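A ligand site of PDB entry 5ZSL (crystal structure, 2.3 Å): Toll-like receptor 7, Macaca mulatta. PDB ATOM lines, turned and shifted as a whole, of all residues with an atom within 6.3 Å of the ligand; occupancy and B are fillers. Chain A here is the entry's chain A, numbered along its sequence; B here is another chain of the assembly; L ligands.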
ATOM      1  N   TYR A 242      10.950  15.356  16.246  1.00  0.00           N
ATOM      2  CA  TYR A 242      11.350  16.294  17.258  1.00  0.00           C
ATOM      3  C   TYR A 242      10.423  17.529  17.237  1.00  0.00           C
ATOM      4  O   TYR A 242      10.286  18.191  16.222  1.00  0.00           O
ATOM      5  CB  TYR A 242      12.817  16.678  17.086  1.00  0.00           C
ATOM      6  CG  TYR A 242      13.360  17.480  18.242  1.00  0.00           C
ATOM      7  CD1 TYR A 242      13.410  16.941  19.527  1.00  0.00           C
ATOM      8  CD2 TYR A 242      13.786  18.780  18.061  1.00  0.00           C
ATOM      9  CE1 TYR A 242      13.897  17.684  20.596  1.00  0.00           C
ATOM     10  CE2 TYR A 242      14.296  19.522  19.122  1.00  0.00           C
ATOM     11  CZ  TYR A 242      14.346  18.975  20.388  1.00  0.00           C
ATOM     12  OH  TYR A 242      14.881  19.703  21.412  1.00  0.00           O
ATOM     13  N   ASN A 243       9.794  17.825  18.383  1.00  0.00           N
ATOM     14  CA  ASN A 243       8.940  19.010  18.618  1.00  0.00           C
ATOM     15  C   ASN A 243       7.732  18.992  17.663  1.00  0.00           C
ATOM     16  O   ASN A 243       7.178  20.024  17.369  1.00  0.00           O
ATOM     17  CB  ASN A 243       9.720  20.321  18.496  1.00  0.00           C
ATOM     18  CG  ASN A 243      10.429  20.686  19.786  1.00  0.00           C
ATOM     19  OD1 ASN A 243       9.959  20.311  20.883  1.00  0.00           O
ATOM     20  ND2 ASN A 243      11.543  21.408  19.677  1.00  0.00           N
ATOM     21  N   PHE A 329      18.883  20.410  11.438  1.00  0.00           N
ATOM     22  CA  PHE A 329      19.892  20.469  12.496  1.00  0.00           C
ATOM     23  C   PHE A 329      19.933  19.168  13.292  1.00  0.00           C
ATOM     24  O   PHE A 329      18.947  18.461  13.424  1.00  0.00           O
ATOM     25  CB  PHE A 329      19.643  21.665  13.425  1.00  0.00           C
ATOM     26  CG  PHE A 329      18.464  21.561  14.387  1.00  0.00           C
ATOM     27  CD1 PHE A 329      17.190  21.959  14.012  1.00  0.00           C
ATOM     28  CD2 PHE A 329      18.652  21.175  15.700  1.00  0.00           C
ATOM     29  CE1 PHE A 329      16.139  21.917  14.910  1.00  0.00           C
ATOM     30  CE2 PHE A 329      17.600  21.137  16.607  1.00  0.00           C
ATOM     31  CZ  PHE A 329      16.344  21.504  16.203  1.00  0.00           C
ATOM     32  N   GLU A 330      21.123  18.862  13.809  1.00  0.00           N
ATOM     33  CA  GLU A 330      21.374  17.750  14.709  1.00  0.00           C
ATOM     34  C   GLU A 330      20.955  18.165  16.122  1.00  0.00           C
ATOM     35  O   GLU A 330      21.370  19.208  16.620  1.00  0.00           O
ATOM     36  CB  GLU A 330      22.864  17.404  14.660  1.00  0.00           C
ATOM     37  CG  GLU A 330      23.233  16.038  15.252  1.00  0.00           C
ATOM     38  CD  GLU A 330      24.703  15.631  15.150  1.00  0.00           C
ATOM     39  OE1 GLU A 330      25.449  16.215  14.294  1.00  0.00           O
ATOM     40  OE2 GLU A 330      25.132  14.732  15.925  1.00  0.00           O
ATOM     41  N   LEU A 331      20.165  17.322  16.782  1.00  0.00           N
ATOM     42  CA  LEU A 331      19.646  17.630  18.093  1.00  0.00           C
ATOM     43  C   LEU A 331      20.833  17.884  19.042  1.00  0.00           C
ATOM     44  O   LEU A 331      21.826  17.180  18.989  1.00  0.00           O
ATOM     45  CB  LEU A 331      18.734  16.498  18.577  1.00  0.00           C
ATOM     46  CG  LEU A 331      17.674  16.013  17.582  1.00  0.00           C
ATOM     47  CD1 LEU A 331      16.708  14.993  18.200  1.00  0.00           C
ATOM     48  CD2 LEU A 331      16.897  17.177  17.000  1.00  0.00           C
ATOM     49  N   GLN A 332      20.718  18.950  19.839  1.00  0.00           N
ATOM     50  CA  GLN A 332      21.708  19.343  20.881  1.00  0.00           C
ATOM     51  C   GLN A 332      23.052  19.744  20.269  1.00  0.00           C
ATOM     52  O   GLN A 332      24.032  19.752  20.954  1.00  0.00           O
ATOM     53  CB  GLN A 332      21.890  18.247  21.946  1.00  0.00           C
ATOM     54  CG  GLN A 332      20.710  18.110  22.911  1.00  0.00           C
ATOM     55  CD  GLN A 332      19.596  17.249  22.349  1.00  0.00           C
ATOM     56  OE1 GLN A 332      19.812  16.128  21.877  1.00  0.00           O
ATOM     57  NE2 GLN A 332      18.379  17.761  22.419  1.00  0.00           N
ATOM     58  N   VAL A 333      23.081  20.124  18.982  1.00  0.00           N
ATOM     59  CA  VAL A 333      24.241  20.667  18.341  1.00  0.00           C
ATOM     60  C   VAL A 333      23.931  22.100  17.887  1.00  0.00           C
ATOM     61  O   VAL A 333      23.021  22.336  17.078  1.00  0.00           O
ATOM     62  CB  VAL A 333      24.706  19.812  17.134  1.00  0.00           C
ATOM     63  CG1 VAL A 333      25.786  20.535  16.323  1.00  0.00           C
ATOM     64  CG2 VAL A 333      25.189  18.436  17.562  1.00  0.00           C
ATOM     65  N   TYR A 334      24.785  23.017  18.334  1.00  0.00           N
ATOM     66  CA  TYR A 334      24.744  24.425  17.993  1.00  0.00           C
ATOM     67  C   TYR A 334      26.044  24.780  17.256  1.00  0.00           C
ATOM     68  O   TYR A 334      27.031  25.173  17.872  1.00  0.00           O
ATOM     69  CB  TYR A 334      24.545  25.205  19.302  1.00  0.00           C
ATOM     70  CG  TYR A 334      24.118  26.659  19.204  1.00  0.00           C
ATOM     71  CD1 TYR A 334      23.757  27.236  17.993  1.00  0.00           C
ATOM     72  CD2 TYR A 334      24.025  27.432  20.347  1.00  0.00           C
ATOM     73  CE1 TYR A 334      23.321  28.549  17.934  1.00  0.00           C
ATOM     74  CE2 TYR A 334      23.585  28.736  20.291  1.00  0.00           C
ATOM     75  CZ  TYR A 334      23.239  29.299  19.088  1.00  0.00           C
ATOM     76  OH  TYR A 334      22.848  30.608  19.065  1.00  0.00           O
ATOM     77  N   VAL A 359      20.597  26.156  12.718  1.00  0.00           N
ATOM     78  CA  VAL A 359      20.918  26.407  14.112  1.00  0.00           C
ATOM     79  C   VAL A 359      22.435  26.601  14.254  1.00  0.00           C
ATOM     80  O   VAL A 359      23.154  25.623  14.447  1.00  0.00           O
ATOM     81  CB  VAL A 359      20.392  25.282  15.040  1.00  0.00           C
ATOM     82  CG1 VAL A 359      20.627  25.612  16.515  1.00  0.00           C
ATOM     83  CG2 VAL A 359      18.935  24.973  14.787  1.00  0.00           C
ATOM     84  N   ASN A 385      17.245  30.276  13.251  1.00  0.00           N
ATOM     85  CA  ASN A 385      18.568  29.703  13.247  1.00  0.00           C
ATOM     86  C   ASN A 385      19.354  30.061  14.511  1.00  0.00           C
ATOM     87  O   ASN A 385      20.459  29.571  14.666  1.00  0.00           O
ATOM     88  CB  ASN A 385      19.379  30.129  12.016  1.00  0.00           C
ATOM     89  CG  ASN A 385      19.167  29.166  10.872  1.00  0.00           C
ATOM     90  OD1 ASN A 385      19.360  27.967  11.054  1.00  0.00           O
ATOM     91  ND2 ASN A 385      18.739  29.669   9.723  1.00  0.00           N
ATOM     92  N   PHE A 386      18.766  30.866  15.395  1.00  0.00           N
ATOM     93  CA  PHE A 386      19.392  31.316  16.643  1.00  0.00           C
ATOM     94  C   PHE A 386      20.767  31.944  16.360  1.00  0.00           C
ATOM     95  O   PHE A 386      21.690  31.854  17.171  1.00  0.00           O
ATOM     96  CB  PHE A 386      19.473  30.167  17.649  1.00  0.00           C
ATOM     97  CG  PHE A 386      18.118  29.566  17.932  1.00  0.00           C
ATOM     98  CD1 PHE A 386      17.298  30.128  18.897  1.00  0.00           C
ATOM     99  CD2 PHE A 386      17.632  28.512  17.172  1.00  0.00           C
ATOM    100  CE1 PHE A 386      16.032  29.608  19.129  1.00  0.00           C
ATOM    101  CE2 PHE A 386      16.366  27.996  17.413  1.00  0.00           C
ATOM    102  CZ  PHE A 386      15.574  28.550  18.384  1.00  0.00           C
ATOM    103  N   LYS A 410      18.758  35.505  17.081  1.00  0.00           N
ATOM    104  CA  LYS A 410      19.263  36.030  18.311  1.00  0.00           C
ATOM    105  C   LYS A 410      20.260  37.155  18.031  1.00  0.00           C
ATOM    106  O   LYS A 410      21.110  37.446  18.858  1.00  0.00           O
ATOM    107  CB  LYS A 410      19.872  34.869  19.100  1.00  0.00           C
ATOM    108  CG  LYS A 410      18.841  33.939  19.708  1.00  0.00           C
ATOM    109  CD  LYS A 410      18.232  34.426  21.002  1.00  0.00           C
ATOM    110  CE  LYS A 410      17.612  33.299  21.806  1.00  0.00           C
ATOM    111  NZ  LYS A 410      16.853  33.805  22.974  1.00  0.00           N
ATOM    112  N   SER B 508      15.879  38.067  27.542  1.00  0.00           N
ATOM    113  CA  SER B 508      15.633  37.202  26.408  1.00  0.00           C
ATOM    114  C   SER B 508      16.530  35.951  26.445  1.00  0.00           C
ATOM    115  O   SER B 508      16.647  35.278  25.456  1.00  0.00           O
ATOM    116  CB  SER B 508      15.879  37.934  25.122  1.00  0.00           C
ATOM    117  OG  SER B 508      14.934  38.986  25.005  1.00  0.00           O
ATOM    118  N   THR B 510      18.353  32.278  27.706  1.00  0.00           N
ATOM    119  CA  THR B 510      18.000  30.899  28.045  1.00  0.00           C
ATOM    120  C   THR B 510      18.432  30.616  29.480  1.00  0.00           C
ATOM    121  O   THR B 510      19.414  29.917  29.708  1.00  0.00           O
ATOM    122  CB  THR B 510      18.641  29.921  27.043  1.00  0.00           C
ATOM    123  OG1 THR B 510      20.012  30.248  26.836  1.00  0.00           O
ATOM    124  CG2 THR B 510      17.997  29.947  25.674  1.00  0.00           C
ATOM    125  N   ASP B 533      13.176  32.646  27.496  1.00  0.00           N
ATOM    126  CA  ASP B 533      13.403  31.521  26.578  1.00  0.00           C
ATOM    127  C   ASP B 533      13.607  30.252  27.414  1.00  0.00           C
ATOM    128  O   ASP B 533      14.709  29.998  27.859  1.00  0.00           O
ATOM    129  CB  ASP B 533      14.608  31.812  25.679  1.00  0.00           C
ATOM    130  CG  ASP B 533      14.797  30.853  24.512  1.00  0.00           C
ATOM    131  OD1 ASP B 533      14.099  29.830  24.459  1.00  0.00           O
ATOM    132  OD2 ASP B 533      15.662  31.164  23.639  1.00  0.00           O
ATOM    133  N   LEU B 534      12.544  29.470  27.596  1.00  0.00           N
ATOM    134  CA  LEU B 534      12.540  28.315  28.479  1.00  0.00           C
ATOM    135  C   LEU B 534      13.136  27.073  27.774  1.00  0.00           C
ATOM    136  O   LEU B 534      12.513  25.993  27.739  1.00  0.00           O
ATOM    137  CB  LEU B 534      11.085  28.009  28.880  1.00  0.00           C
ATOM    138  CG  LEU B 534      10.735  28.045  30.362  1.00  0.00           C
ATOM    139  CD1 LEU B 534       9.469  27.266  30.608  1.00  0.00           C
ATOM    140  CD2 LEU B 534      11.847  27.554  31.249  1.00  0.00           C
ATOM    141  N   LEU B 535      14.348  27.202  27.241  1.00  0.00           N
ATOM    142  CA  LEU B 535      15.045  26.088  26.607  1.00  0.00           C
ATOM    143  C   LEU B 535      15.462  25.057  27.667  1.00  0.00           C
ATOM    144  O   LEU B 535      15.399  23.858  27.409  1.00  0.00           O
ATOM    145  CB  LEU B 535      16.281  26.608  25.871  1.00  0.00           C
ATOM    146  CG  LEU B 535      17.270  25.540  25.408  1.00  0.00           C
ATOM    147  CD1 LEU B 535      16.619  24.546  24.493  1.00  0.00           C
ATOM    148  CD2 LEU B 535      18.459  26.177  24.717  1.00  0.00           C
ATOM    149  N   TYR B 557       8.828  33.996  22.583  1.00  0.00           N
ATOM    150  CA  TYR B 557       9.443  32.817  21.994  1.00  0.00           C
ATOM    151  C   TYR B 557       8.428  31.657  21.863  1.00  0.00           C
ATOM    152  O   TYR B 557       8.669  30.701  21.145  1.00  0.00           O
ATOM    153  CB  TYR B 557      10.692  32.426  22.780  1.00  0.00           C
ATOM    154  CG  TYR B 557      11.862  33.357  22.616  1.00  0.00           C
ATOM    155  CD1 TYR B 557      12.476  33.558  21.373  1.00  0.00           C
ATOM    156  CD2 TYR B 557      12.388  34.006  23.717  1.00  0.00           C
ATOM    157  CE1 TYR B 557      13.555  34.420  21.234  1.00  0.00           C
ATOM    158  CE2 TYR B 557      13.466  34.876  23.596  1.00  0.00           C
ATOM    159  CZ  TYR B 557      14.039  35.080  22.350  1.00  0.00           C
ATOM    160  OH  TYR B 557      15.087  35.933  22.300  1.00  0.00           O
ATOM    161  N   GLY B 562       8.870  25.556  16.207  1.00  0.00           N
ATOM    162  CA  GLY B 562      10.123  24.851  16.180  1.00  0.00           C
ATOM    163  C   GLY B 562      11.044  25.256  17.322  1.00  0.00           C
ATOM    164  O   GLY B 562      12.253  24.916  17.298  1.00  0.00           O
ATOM    165  N   ILE B 563      10.519  25.986  18.308  1.00  0.00           N
ATOM    166  CA  ILE B 563      11.365  26.373  19.420  1.00  0.00           C
ATOM    167  C   ILE B 563      11.066  25.447  20.603  1.00  0.00           C
ATOM    168  O   ILE B 563       9.929  25.271  21.009  1.00  0.00           O
ATOM    169  CB  ILE B 563      11.209  27.857  19.794  1.00  0.00           C
ATOM    170  CG1 ILE B 563      11.463  28.778  18.611  1.00  0.00           C
ATOM    171  CG2 ILE B 563      12.121  28.215  20.955  1.00  0.00           C
ATOM    172  CD1 ILE B 563      11.551  30.250  19.024  1.00  0.00           C
ATOM    173  N   THR B 564      12.137  24.900  21.173  1.00  0.00           N
ATOM    174  CA  THR B 564      12.104  24.011  22.311  1.00  0.00           C
ATOM    175  C   THR B 564      11.815  24.792  23.593  1.00  0.00           C
ATOM    176  O   THR B 564      12.531  25.700  23.916  1.00  0.00           O
ATOM    177  CB  THR B 564      13.434  23.232  22.374  1.00  0.00           C
ATOM    178  OG1 THR B 564      13.404  22.440  21.178  1.00  0.00           O
ATOM    179  CG2 THR B 564      13.596  22.329  23.583  1.00  0.00           C
ATOM    180  N   HIS B 565      10.771  24.362  24.311  1.00  0.00           N
ATOM    181  CA  HIS B 565      10.378  24.891  25.609  1.00  0.00           C
ATOM    182  C   HIS B 565      10.231  23.726  26.609  1.00  0.00           C
ATOM    183  O   HIS B 565       9.563  22.753  26.317  1.00  0.00           O
ATOM    184  CB  HIS B 565       9.026  25.630  25.540  1.00  0.00           C
ATOM    185  CG  HIS B 565       8.784  26.449  24.330  1.00  0.00           C
ATOM    186  ND1 HIS B 565       9.518  27.590  24.061  1.00  0.00           N
ATOM    187  CD2 HIS B 565       7.843  26.349  23.349  1.00  0.00           C
ATOM    188  CE1 HIS B 565       9.072  28.128  22.951  1.00  0.00           C
ATOM    189  NE2 HIS B 565       8.051  27.385  22.485  1.00  0.00           N
HETATM  190  O1  LIG L   1      18.896  30.473  22.450  1.00  0.00           O
HETATM  191  C1  LIG L   1      18.351  29.409  22.140  1.00  0.00           C
HETATM  192  C2  LIG L   1      19.068  28.360  21.402  1.00  0.00           C
HETATM  193  N1  LIG L   1      20.313  28.180  20.906  1.00  0.00           N
HETATM  194  C3  LIG L   1      20.300  26.944  20.328  1.00  0.00           C
HETATM  195  N2  LIG L   1      17.067  29.224  22.465  1.00  0.00           N
HETATM  196  C4  LIG L   1      16.412  28.109  22.148  1.00  0.00           C
HETATM  197  N3  LIG L   1      15.123  28.025  22.549  1.00  0.00           N
HETATM  198  N4  LIG L   1      16.983  27.070  21.463  1.00  0.00           N
HETATM  199  C5  LIG L   1      18.271  27.158  21.072  1.00  0.00           C
HETATM  200  N5  LIG L   1      19.090  26.342  20.413  1.00  0.00           N
HETATM  201  C6  LIG L   1      18.683  25.005  19.879  1.00  0.00           C
HETATM  202  C7  LIG L   1      18.198  24.093  21.001  1.00  0.00           C
HETATM  203  O2  LIG L   1      19.022  23.000  21.238  1.00  0.00           O
HETATM  204  O3  LIG L   1      17.566  25.129  18.966  1.00  0.00           O
HETATM  205  C8  LIG L   1      16.645  24.044  19.134  1.00  0.00           C
HETATM  206  C9  LIG L   1      15.230  24.529  18.921  1.00  0.00           C
HETATM  207  O4  LIG L   1      14.962  25.662  19.789  1.00  0.00           O
HETATM  208  C10 LIG L   1      16.855  23.557  20.558  1.00  0.00           C
HETATM  209  O5  LIG L   1      16.843  22.151  20.688  1.00  0.00           O
HETATM  210  P1  LIG L   1      18.263  21.624  21.139  1.00  0.00           P
HETATM  211  O6  LIG L   1      18.222  20.975  22.488  1.00  0.00           O
HETATM  212  O7  LIG L   1      18.734  20.748  20.028  1.00  0.00           O
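The side-chain carboxylate (OD2) of Asp 533 of chain B is in salt-bridge range of the side-chain amino group (NZ) of Lys 410, 3.0 Å away.
The side-chain amino group (NZ) of Lys 410 is in hydrogen-bond range of the backbone carbonyl oxygen (O) of Ser 508 of chain B (2.9 Å).
The side-chain amino group of Lys 410 lies within hydrogen-bond range of the side-chain hydroxyl of Tyr 557 of chain B (2.8 Å).
The side-chain hydroxyl (OH) of Tyr 242 lies within hydrogen-bond range of the side-chain hydroxyl (OG1) of Thr 564 of chain B.
The side-chain amide nitrogen (ND2) of Asn 243 sits at hydrogen-bond distance from the side-chain hydroxyl (OG1) of Thr 564 of chain B (2.6 Å).
OH of Tyr 334 is in hydrogen-bond range of O of Phe 386 (2.5 Å).
A ring nitrogen (NE2) of His 565 of chain B lies within hydrogen-bond range of the backbone carbonyl oxygen (O) of Ile 563 of chain B, at 3.2 Å.
The backbone NH of Val 359 is in hydrogen-bond range of the side-chain amide oxygen of Asn 385 (2.8 Å).
Residues that only touch the ligand: Lys 410 (3.2 Å), Phe 386 (3.3 Å), Tyr 334 (3.4 Å), Thr 510 of chain B (3.4 Å), Ile 563 of chain B (3.4 Å), Gly 562 of chain B (3.4 Å), Phe 329 (3.6 Å), Leu 535 of chain B (3.7 Å), Leu 331 (3.7 Å) and Val 359 (3.9 Å).
A nitrogen (N2) of the ligand sits at hydrogen-bond distance from the side-chain carboxylate (OD2) of Asp 533 of chain B, 2.7 Å away.
O7 of the ligand lies within hydrogen-bond range of N of Gln 332.
NE2 of Gln 332 is in hydrogen-bond range of O6 of the ligand (3.2 Å).
OH of Tyr 242 is in hydrogen-bond range of O5 of the ligand (3.2 Å).
O4 of the ligand lies within hydrogen-bond range of N of Thr 564 of chain B (3.2 Å).
The side-chain hydroxyl of Thr 564 of chain B sits at hydrogen-bond distance from an oxygen (O5) of the ligand (3.5 Å).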
